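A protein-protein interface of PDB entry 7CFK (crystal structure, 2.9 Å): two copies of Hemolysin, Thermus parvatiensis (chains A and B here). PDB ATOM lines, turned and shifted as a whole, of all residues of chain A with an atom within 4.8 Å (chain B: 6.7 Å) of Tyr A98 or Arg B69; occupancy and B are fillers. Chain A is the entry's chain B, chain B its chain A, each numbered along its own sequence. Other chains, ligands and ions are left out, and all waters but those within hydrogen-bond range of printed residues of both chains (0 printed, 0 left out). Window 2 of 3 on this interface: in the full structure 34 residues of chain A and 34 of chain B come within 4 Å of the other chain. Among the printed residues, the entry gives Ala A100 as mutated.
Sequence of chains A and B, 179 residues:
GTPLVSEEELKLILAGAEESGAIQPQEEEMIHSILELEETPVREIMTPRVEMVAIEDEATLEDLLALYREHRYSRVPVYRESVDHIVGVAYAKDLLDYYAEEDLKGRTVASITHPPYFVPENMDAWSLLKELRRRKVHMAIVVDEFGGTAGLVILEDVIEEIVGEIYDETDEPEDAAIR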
ATOM      1  N   LEU A  61       9.501  -0.252  26.515  1.00  0.00           N
ATOM      2  CA  LEU A  61      10.621   0.314  27.253  1.00  0.00           C
ATOM      3  C   LEU A  61      10.501   0.067  28.751  1.00  0.00           C
ATOM      4  O   LEU A  61      11.528   0.037  29.454  1.00  0.00           O
ATOM      5  CB  LEU A  61      10.725   1.810  26.955  1.00  0.00           C
ATOM      6  CG  LEU A  61      11.562   2.299  25.761  1.00  0.00           C
ATOM      7  CD1 LEU A  61      11.362   1.490  24.484  1.00  0.00           C
ATOM      8  CD2 LEU A  61      11.205   3.735  25.498  1.00  0.00           C
ATOM      9  N   ASP A  94      19.702   4.950  27.490  1.00  0.00           N
ATOM     10  CA  ASP A  94      18.821   5.707  26.619  1.00  0.00           C
ATOM     11  C   ASP A  94      17.445   5.860  27.239  1.00  0.00           C
ATOM     12  O   ASP A  94      16.757   6.861  26.981  1.00  0.00           O
ATOM     13  CB  ASP A  94      18.769   5.042  25.241  1.00  0.00           C
ATOM     14  CG  ASP A  94      19.992   5.413  24.357  1.00  0.00           C
ATOM     15  OD1 ASP A  94      21.099   5.618  24.907  1.00  0.00           O
ATOM     16  OD2 ASP A  94      19.863   5.503  23.111  1.00  0.00           O
ATOM     17  N   LEU A  95      17.073   4.928  28.122  1.00  0.00           N
ATOM     18  CA  LEU A  95      15.859   5.083  28.916  1.00  0.00           C
ATOM     19  C   LEU A  95      15.808   6.437  29.607  1.00  0.00           C
ATOM     20  O   LEU A  95      14.744   7.061  29.683  1.00  0.00           O
ATOM     21  CB  LEU A  95      15.781   3.974  29.959  1.00  0.00           C
ATOM     22  CG  LEU A  95      15.642   2.588  29.385  1.00  0.00           C
ATOM     23  CD1 LEU A  95      15.331   1.658  30.521  1.00  0.00           C
ATOM     24  CD2 LEU A  95      14.538   2.610  28.374  1.00  0.00           C
ATOM     25  N   LEU A  96      16.954   6.900  30.118  1.00  0.00           N
ATOM     26  CA  LEU A  96      17.005   8.148  30.864  1.00  0.00           C
ATOM     27  C   LEU A  96      16.467   9.327  30.056  1.00  0.00           C
ATOM     28  O   LEU A  96      15.841  10.231  30.622  1.00  0.00           O
ATOM     29  CB  LEU A  96      18.440   8.401  31.295  1.00  0.00           C
ATOM     30  CG  LEU A  96      18.990   7.346  32.244  1.00  0.00           C
ATOM     31  CD1 LEU A  96      20.434   7.651  32.590  1.00  0.00           C
ATOM     32  CD2 LEU A  96      18.153   7.319  33.501  1.00  0.00           C
ATOM     33  N   ASP A  97      16.668   9.333  28.735  1.00  0.00           N
ATOM     34  CA  ASP A  97      16.134  10.438  27.946  1.00  0.00           C
ATOM     35  C   ASP A  97      14.611  10.480  27.974  1.00  0.00           C
ATOM     36  O   ASP A  97      14.022  11.527  27.703  1.00  0.00           O
ATOM     37  CB  ASP A  97      16.622  10.343  26.506  1.00  0.00           C
ATOM     38  CG  ASP A  97      18.131  10.401  26.406  1.00  0.00           C
ATOM     39  OD1 ASP A  97      18.753  10.975  27.336  1.00  0.00           O
ATOM     40  OD2 ASP A  97      18.689   9.864  25.413  1.00  0.00           O
ATOM     41  N   TYR A  98      13.958   9.362  28.270  1.00  0.00           N
ATOM     42  CA  TYR A  98      12.511   9.328  28.437  1.00  0.00           C
ATOM     43  C   TYR A  98      12.150   9.359  29.918  1.00  0.00           C
ATOM     44  O   TYR A  98      11.424  10.255  30.369  1.00  0.00           O
ATOM     45  CB  TYR A  98      11.927   8.063  27.780  1.00  0.00           C
ATOM     46  CG  TYR A  98      12.002   7.986  26.264  1.00  0.00           C
ATOM     47  CD1 TYR A  98      13.207   7.784  25.610  1.00  0.00           C
ATOM     48  CD2 TYR A  98      10.852   8.115  25.491  1.00  0.00           C
ATOM     49  CE1 TYR A  98      13.267   7.712  24.237  1.00  0.00           C
ATOM     50  CE2 TYR A  98      10.903   8.038  24.114  1.00  0.00           C
ATOM     51  CZ  TYR A  98      12.120   7.835  23.496  1.00  0.00           C
ATOM     52  OH  TYR A  98      12.175   7.766  22.123  1.00  0.00           O
ATOM     53  N   TYR A  99      12.615   8.342  30.665  1.00  0.00           N
ATOM     54  CA  TYR A  99      12.573   8.206  32.124  1.00  0.00           C
ATOM     55  C   TYR A  99      11.257   8.696  32.723  1.00  0.00           C
ATOM     56  O   TYR A  99      11.223   9.179  33.860  1.00  0.00           O
ATOM     57  CB  TYR A  99      13.762   8.929  32.759  1.00  0.00           C
ATOM     58  N   ALA A 100      10.163   8.555  31.984  1.00  0.00           N
ATOM     59  CA  ALA A 100       8.856   9.036  32.411  1.00  0.00           C
ATOM     60  C   ALA A 100       7.942   7.824  32.535  1.00  0.00           C
ATOM     61  O   ALA A 100       7.589   7.207  31.523  1.00  0.00           O
ATOM     62  CB  ALA A 100       8.300  10.072  31.428  1.00  0.00           C
ATOM     63  N   ASP A 103       5.849   7.673  29.636  1.00  0.00           N
ATOM     64  CA  ASP A 103       6.305   7.477  28.269  1.00  0.00           C
ATOM     65  C   ASP A 103       6.847   6.065  28.042  1.00  0.00           C
ATOM     66  O   ASP A 103       6.807   5.561  26.913  1.00  0.00           O
ATOM     67  CB  ASP A 103       7.361   8.535  27.921  1.00  0.00           C
ATOM     68  N   LEU A 104       7.361   5.412  29.087  1.00  0.00           N
ATOM     69  CA  LEU A 104       8.108   4.175  28.877  1.00  0.00           C
ATOM     70  C   LEU A 104       7.211   3.043  28.380  1.00  0.00           C
ATOM     71  O   LEU A 104       7.508   2.416  27.357  1.00  0.00           O
ATOM     72  CB  LEU A 104       8.836   3.775  30.156  1.00  0.00           C
ATOM     73  CG  LEU A 104      10.080   4.641  30.359  1.00  0.00           C
ATOM     74  CD1 LEU A 104      11.056   4.035  31.362  1.00  0.00           C
ATOM     75  CD2 LEU A 104      10.766   4.937  29.024  1.00  0.00           C
ATOM     76  N   SER A 111      11.997   1.456  19.035  1.00  0.00           N
ATOM     77  CA  SER A 111      12.157   2.893  18.803  1.00  0.00           C
ATOM     78  C   SER A 111      13.521   3.420  19.243  1.00  0.00           C
ATOM     79  O   SER A 111      13.831   4.572  18.939  1.00  0.00           O
ATOM     80  CB  SER A 111      11.035   3.705  19.484  1.00  0.00           C
ATOM     81  OG  SER A 111      11.336   4.114  20.813  1.00  0.00           O
ATOM     82  N   ILE A 112      14.340   2.622  19.937  1.00  0.00           N
ATOM     83  CA  ILE A 112      15.655   3.074  20.392  1.00  0.00           C
ATOM     84  C   ILE A 112      16.746   2.073  20.000  1.00  0.00           C
ATOM     85  O   ILE A 112      17.838   2.051  20.582  1.00  0.00           O
ATOM     86  CB  ILE A 112      15.644   3.308  21.914  1.00  0.00           C
ATOM     87  CG1 ILE A 112      15.346   2.003  22.659  1.00  0.00           C
ATOM     88  CG2 ILE A 112      14.599   4.306  22.261  1.00  0.00           C
ATOM     89  CD1 ILE A 112      16.019   1.899  24.009  1.00  0.00           C
ATOM     90  N   LEU B  64      19.533  15.614  39.405  1.00  0.00           N
ATOM     91  CA  LEU B  64      20.585  14.819  38.775  1.00  0.00           C
ATOM     92  C   LEU B  64      20.202  14.452  37.356  1.00  0.00           C
ATOM     93  O   LEU B  64      20.985  14.657  36.423  1.00  0.00           O
ATOM     94  CB  LEU B  64      20.866  13.548  39.576  1.00  0.00           C
ATOM     95  CG  LEU B  64      22.044  12.775  38.991  1.00  0.00           C
ATOM     96  CD1 LEU B  64      23.205  13.694  38.877  1.00  0.00           C
ATOM     97  CD2 LEU B  64      22.421  11.579  39.841  1.00  0.00           C
ATOM     98  N   LEU B  65      18.982  13.930  37.176  1.00  0.00           N
ATOM     99  CA  LEU B  65      18.507  13.550  35.849  1.00  0.00           C
ATOM    100  C   LEU B  65      18.470  14.738  34.902  1.00  0.00           C
ATOM    101  O   LEU B  65      18.796  14.602  33.717  1.00  0.00           O
ATOM    102  CB  LEU B  65      17.124  12.927  35.944  1.00  0.00           C
ATOM    103  CG  LEU B  65      16.651  12.380  34.599  1.00  0.00           C
ATOM    104  CD1 LEU B  65      17.149  10.960  34.432  1.00  0.00           C
ATOM    105  CD2 LEU B  65      15.133  12.425  34.481  1.00  0.00           C
ATOM    106  N   ALA B  66      18.043  15.906  35.394  1.00  0.00           N
ATOM    107  CA  ALA B  66      18.006  17.088  34.541  1.00  0.00           C
ATOM    108  C   ALA B  66      19.403  17.477  34.098  1.00  0.00           C
ATOM    109  O   ALA B  66      19.619  17.849  32.937  1.00  0.00           O
ATOM    110  CB  ALA B  66      17.344  18.248  35.276  1.00  0.00           C
ATOM    111  N   LEU B  67      20.363  17.408  35.024  1.00  0.00           N
ATOM    112  CA  LEU B  67      21.758  17.642  34.674  1.00  0.00           C
ATOM    113  C   LEU B  67      22.186  16.687  33.584  1.00  0.00           C
ATOM    114  O   LEU B  67      22.748  17.101  32.562  1.00  0.00           O
ATOM    115  CB  LEU B  67      22.649  17.476  35.902  1.00  0.00           C
ATOM    116  CG  LEU B  67      24.096  17.958  35.797  1.00  0.00           C
ATOM    117  CD1 LEU B  67      24.161  19.368  35.303  1.00  0.00           C
ATOM    118  CD2 LEU B  67      24.790  17.857  37.142  1.00  0.00           C
ATOM    119  N   TYR B  68      21.879  15.402  33.765  1.00  0.00           N
ATOM    120  CA  TYR B  68      22.291  14.404  32.792  1.00  0.00           C
ATOM    121  C   TYR B  68      21.713  14.714  31.425  1.00  0.00           C
ATOM    122  O   TYR B  68      22.401  14.589  30.408  1.00  0.00           O
ATOM    123  CB  TYR B  68      21.867  13.004  33.233  1.00  0.00           C
ATOM    124  CG  TYR B  68      22.118  11.989  32.153  1.00  0.00           C
ATOM    125  CD1 TYR B  68      23.323  11.306  32.083  1.00  0.00           C
ATOM    126  CD2 TYR B  68      21.160  11.735  31.178  1.00  0.00           C
ATOM    127  CE1 TYR B  68      23.561  10.402  31.082  1.00  0.00           C
ATOM    128  CE2 TYR B  68      21.392  10.842  30.177  1.00  0.00           C
ATOM    129  CZ  TYR B  68      22.590  10.182  30.135  1.00  0.00           C
ATOM    130  OH  TYR B  68      22.796   9.302  29.126  1.00  0.00           O
ATOM    131  N   ARG B  69      20.443  15.097  31.381  1.00  0.00           N
ATOM    132  CA  ARG B  69      19.834  15.487  30.118  1.00  0.00           C
ATOM    133  C   ARG B  69      20.576  16.660  29.494  1.00  0.00           C
ATOM    134  O   ARG B  69      20.863  16.660  28.294  1.00  0.00           O
ATOM    135  CB  ARG B  69      18.375  15.871  30.341  1.00  0.00           C
ATOM    136  CG  ARG B  69      17.518  14.808  30.941  1.00  0.00           C
ATOM    137  CD  ARG B  69      16.081  15.292  31.058  1.00  0.00           C
ATOM    138  NE  ARG B  69      15.232  14.173  31.432  1.00  0.00           N
ATOM    139  CZ  ARG B  69      15.007  13.137  30.636  1.00  0.00           C
ATOM    140  NH1 ARG B  69      15.547  13.117  29.423  1.00  0.00           N
ATOM    141  NH2 ARG B  69      14.244  12.128  31.041  1.00  0.00           N
ATOM    142  N   GLU B  70      20.884  17.682  30.301  1.00  0.00           N
ATOM    143  CA  GLU B  70      21.453  18.906  29.753  1.00  0.00           C
ATOM    144  C   GLU B  70      22.911  18.757  29.351  1.00  0.00           C
ATOM    145  O   GLU B  70      23.415  19.613  28.616  1.00  0.00           O
ATOM    146  CB  GLU B  70      21.318  20.048  30.759  1.00  0.00           C
ATOM    147  N   HIS B  71      23.612  17.718  29.828  1.00  0.00           N
ATOM    148  CA  HIS B  71      25.055  17.631  29.603  1.00  0.00           C
ATOM    149  C   HIS B  71      25.613  16.255  29.241  1.00  0.00           C
ATOM    150  O   HIS B  71      26.785  16.180  28.864  1.00  0.00           O
ATOM    151  CB  HIS B  71      25.803  18.157  30.837  1.00  0.00           C
ATOM    152  CG  HIS B  71      25.540  19.603  31.133  1.00  0.00           C
ATOM    153  ND1 HIS B  71      24.405  20.037  31.786  1.00  0.00           N
ATOM    154  CD2 HIS B  71      26.264  20.714  30.863  1.00  0.00           C
ATOM    155  CE1 HIS B  71      24.441  21.352  31.907  1.00  0.00           C
ATOM    156  NE2 HIS B  71      25.562  21.787  31.360  1.00  0.00           N
ATOM    157  N   ARG B  72      24.853  15.173  29.375  1.00  0.00           N
ATOM    158  CA  ARG B  72      25.187  13.832  28.887  1.00  0.00           C
ATOM    159  C   ARG B  72      26.333  13.164  29.644  1.00  0.00           C
ATOM    160  O   ARG B  72      26.849  12.147  29.184  1.00  0.00           O
ATOM    161  CB  ARG B  72      25.541  13.821  27.396  1.00  0.00           C
ATOM    162  CG  ARG B  72      24.546  14.496  26.471  1.00  0.00           C
ATOM    163  CD  ARG B  72      23.125  14.228  26.879  1.00  0.00           C
ATOM    164  NE  ARG B  72      22.721  12.882  26.493  1.00  0.00           N
ATOM    165  CZ  ARG B  72      21.459  12.501  26.331  1.00  0.00           C
ATOM    166  NH1 ARG B  72      20.477  13.385  26.522  1.00  0.00           N
ATOM    167  NH2 ARG B  72      21.189  11.241  25.984  1.00  0.00           N
ATOM    168  N   TYR B  73      26.739  13.668  30.803  1.00  0.00           N
ATOM    169  CA  TYR B  73      27.824  13.038  31.548  1.00  0.00           C
ATOM    170  C   TYR B  73      27.282  12.017  32.539  1.00  0.00           C
ATOM    171  O   TYR B  73      26.506  12.368  33.428  1.00  0.00           O
ATOM    172  CB  TYR B  73      28.685  14.076  32.258  1.00  0.00           C
ATOM    173  CG  TYR B  73      29.539  14.825  31.286  1.00  0.00           C
ATOM    174  CD1 TYR B  73      30.367  14.140  30.406  1.00  0.00           C
ATOM    175  CD2 TYR B  73      29.506  16.215  31.227  1.00  0.00           C
ATOM    176  CE1 TYR B  73      31.147  14.827  29.499  1.00  0.00           C
ATOM    177  CE2 TYR B  73      30.285  16.905  30.327  1.00  0.00           C
ATOM    178  CZ  TYR B  73      31.103  16.214  29.467  1.00  0.00           C
ATOM    179  OH  TYR B  73      31.872  16.903  28.562  1.00  0.00           O
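Of the 10 printed residues of chain B, 4 touch a printed residue of chain A. Printed residues of chain B that touch a printed residue of chain A: Leu B65, Tyr B68, Arg B69 and Arg B72. Of the 12 printed residues of chain A, 4 touch a printed residue of chain B. Hydrophobic or aromatic side chains of chain A that line the printed part of chain B: Leu A96 and Tyr A99. Among the printed residues, 8 pairs touch across the chains. Among the printed residues, Asp or Glu carboxylates within 4 Å of a Lys or Arg side-chain nitrogen of the other chain: Asp A97 with Arg B72 (2.8 Å).
The backbone carbonyl oxygen (O) of Leu A96 sits at hydrogen-bond distance from the guanidinium group (NH2) of Arg B69 (2.5 Å). O of Asp A97 lies within hydrogen-bond range of NH1 of Arg B69 (2.8 Å). NH2 of Arg B69 sits at hydrogen-bond distance from O of Tyr A98. The guanidinium group (NH2) of Arg B72 is in salt-bridge range of the side-chain carboxylate (OD1) of Asp A97 (2.8 Å).
Asp A94 touches none of the printed residues of chain B. Printed residues of chain B within 4 Å of Leu A96: Leu B65 (3.9 Å), Tyr B68 (3.99 Å) and Arg B69 (2.5 Å). Of the printed residues of chain B, Asp A97 touches Tyr B68, Arg B69 and Arg B72. Of the printed residues of chain B, Tyr A98 touches Arg B69. Asp A103 touches none of the printed residues of chain B. Printed residues of chain A within 4 Å of Leu B65: Leu A96 (3.9 Å). Of the printed residues of chain A, Tyr B68 touches Leu A96 (3.99 Å) and Asp A97 (3.9 Å). Arg B69 touches four residues of chain A. The nearest printed residue of chain A that does not touch Arg B69 is Leu A95 (5.3 Å).
Among the printed residues, pairs that only touch across the chains: Leu A96 with Leu B65 (3.9 Å), Leu A96 with Tyr B68 (3.99 Å), Asp A97 with Tyr B68 (3.9 Å) and Tyr A99 with Arg B69 (3.7 Å).
No position is printed for both chains. Of the 8 pairs that touch across the chains among the printed residues, none has its exchanged pair printed and touching as well.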
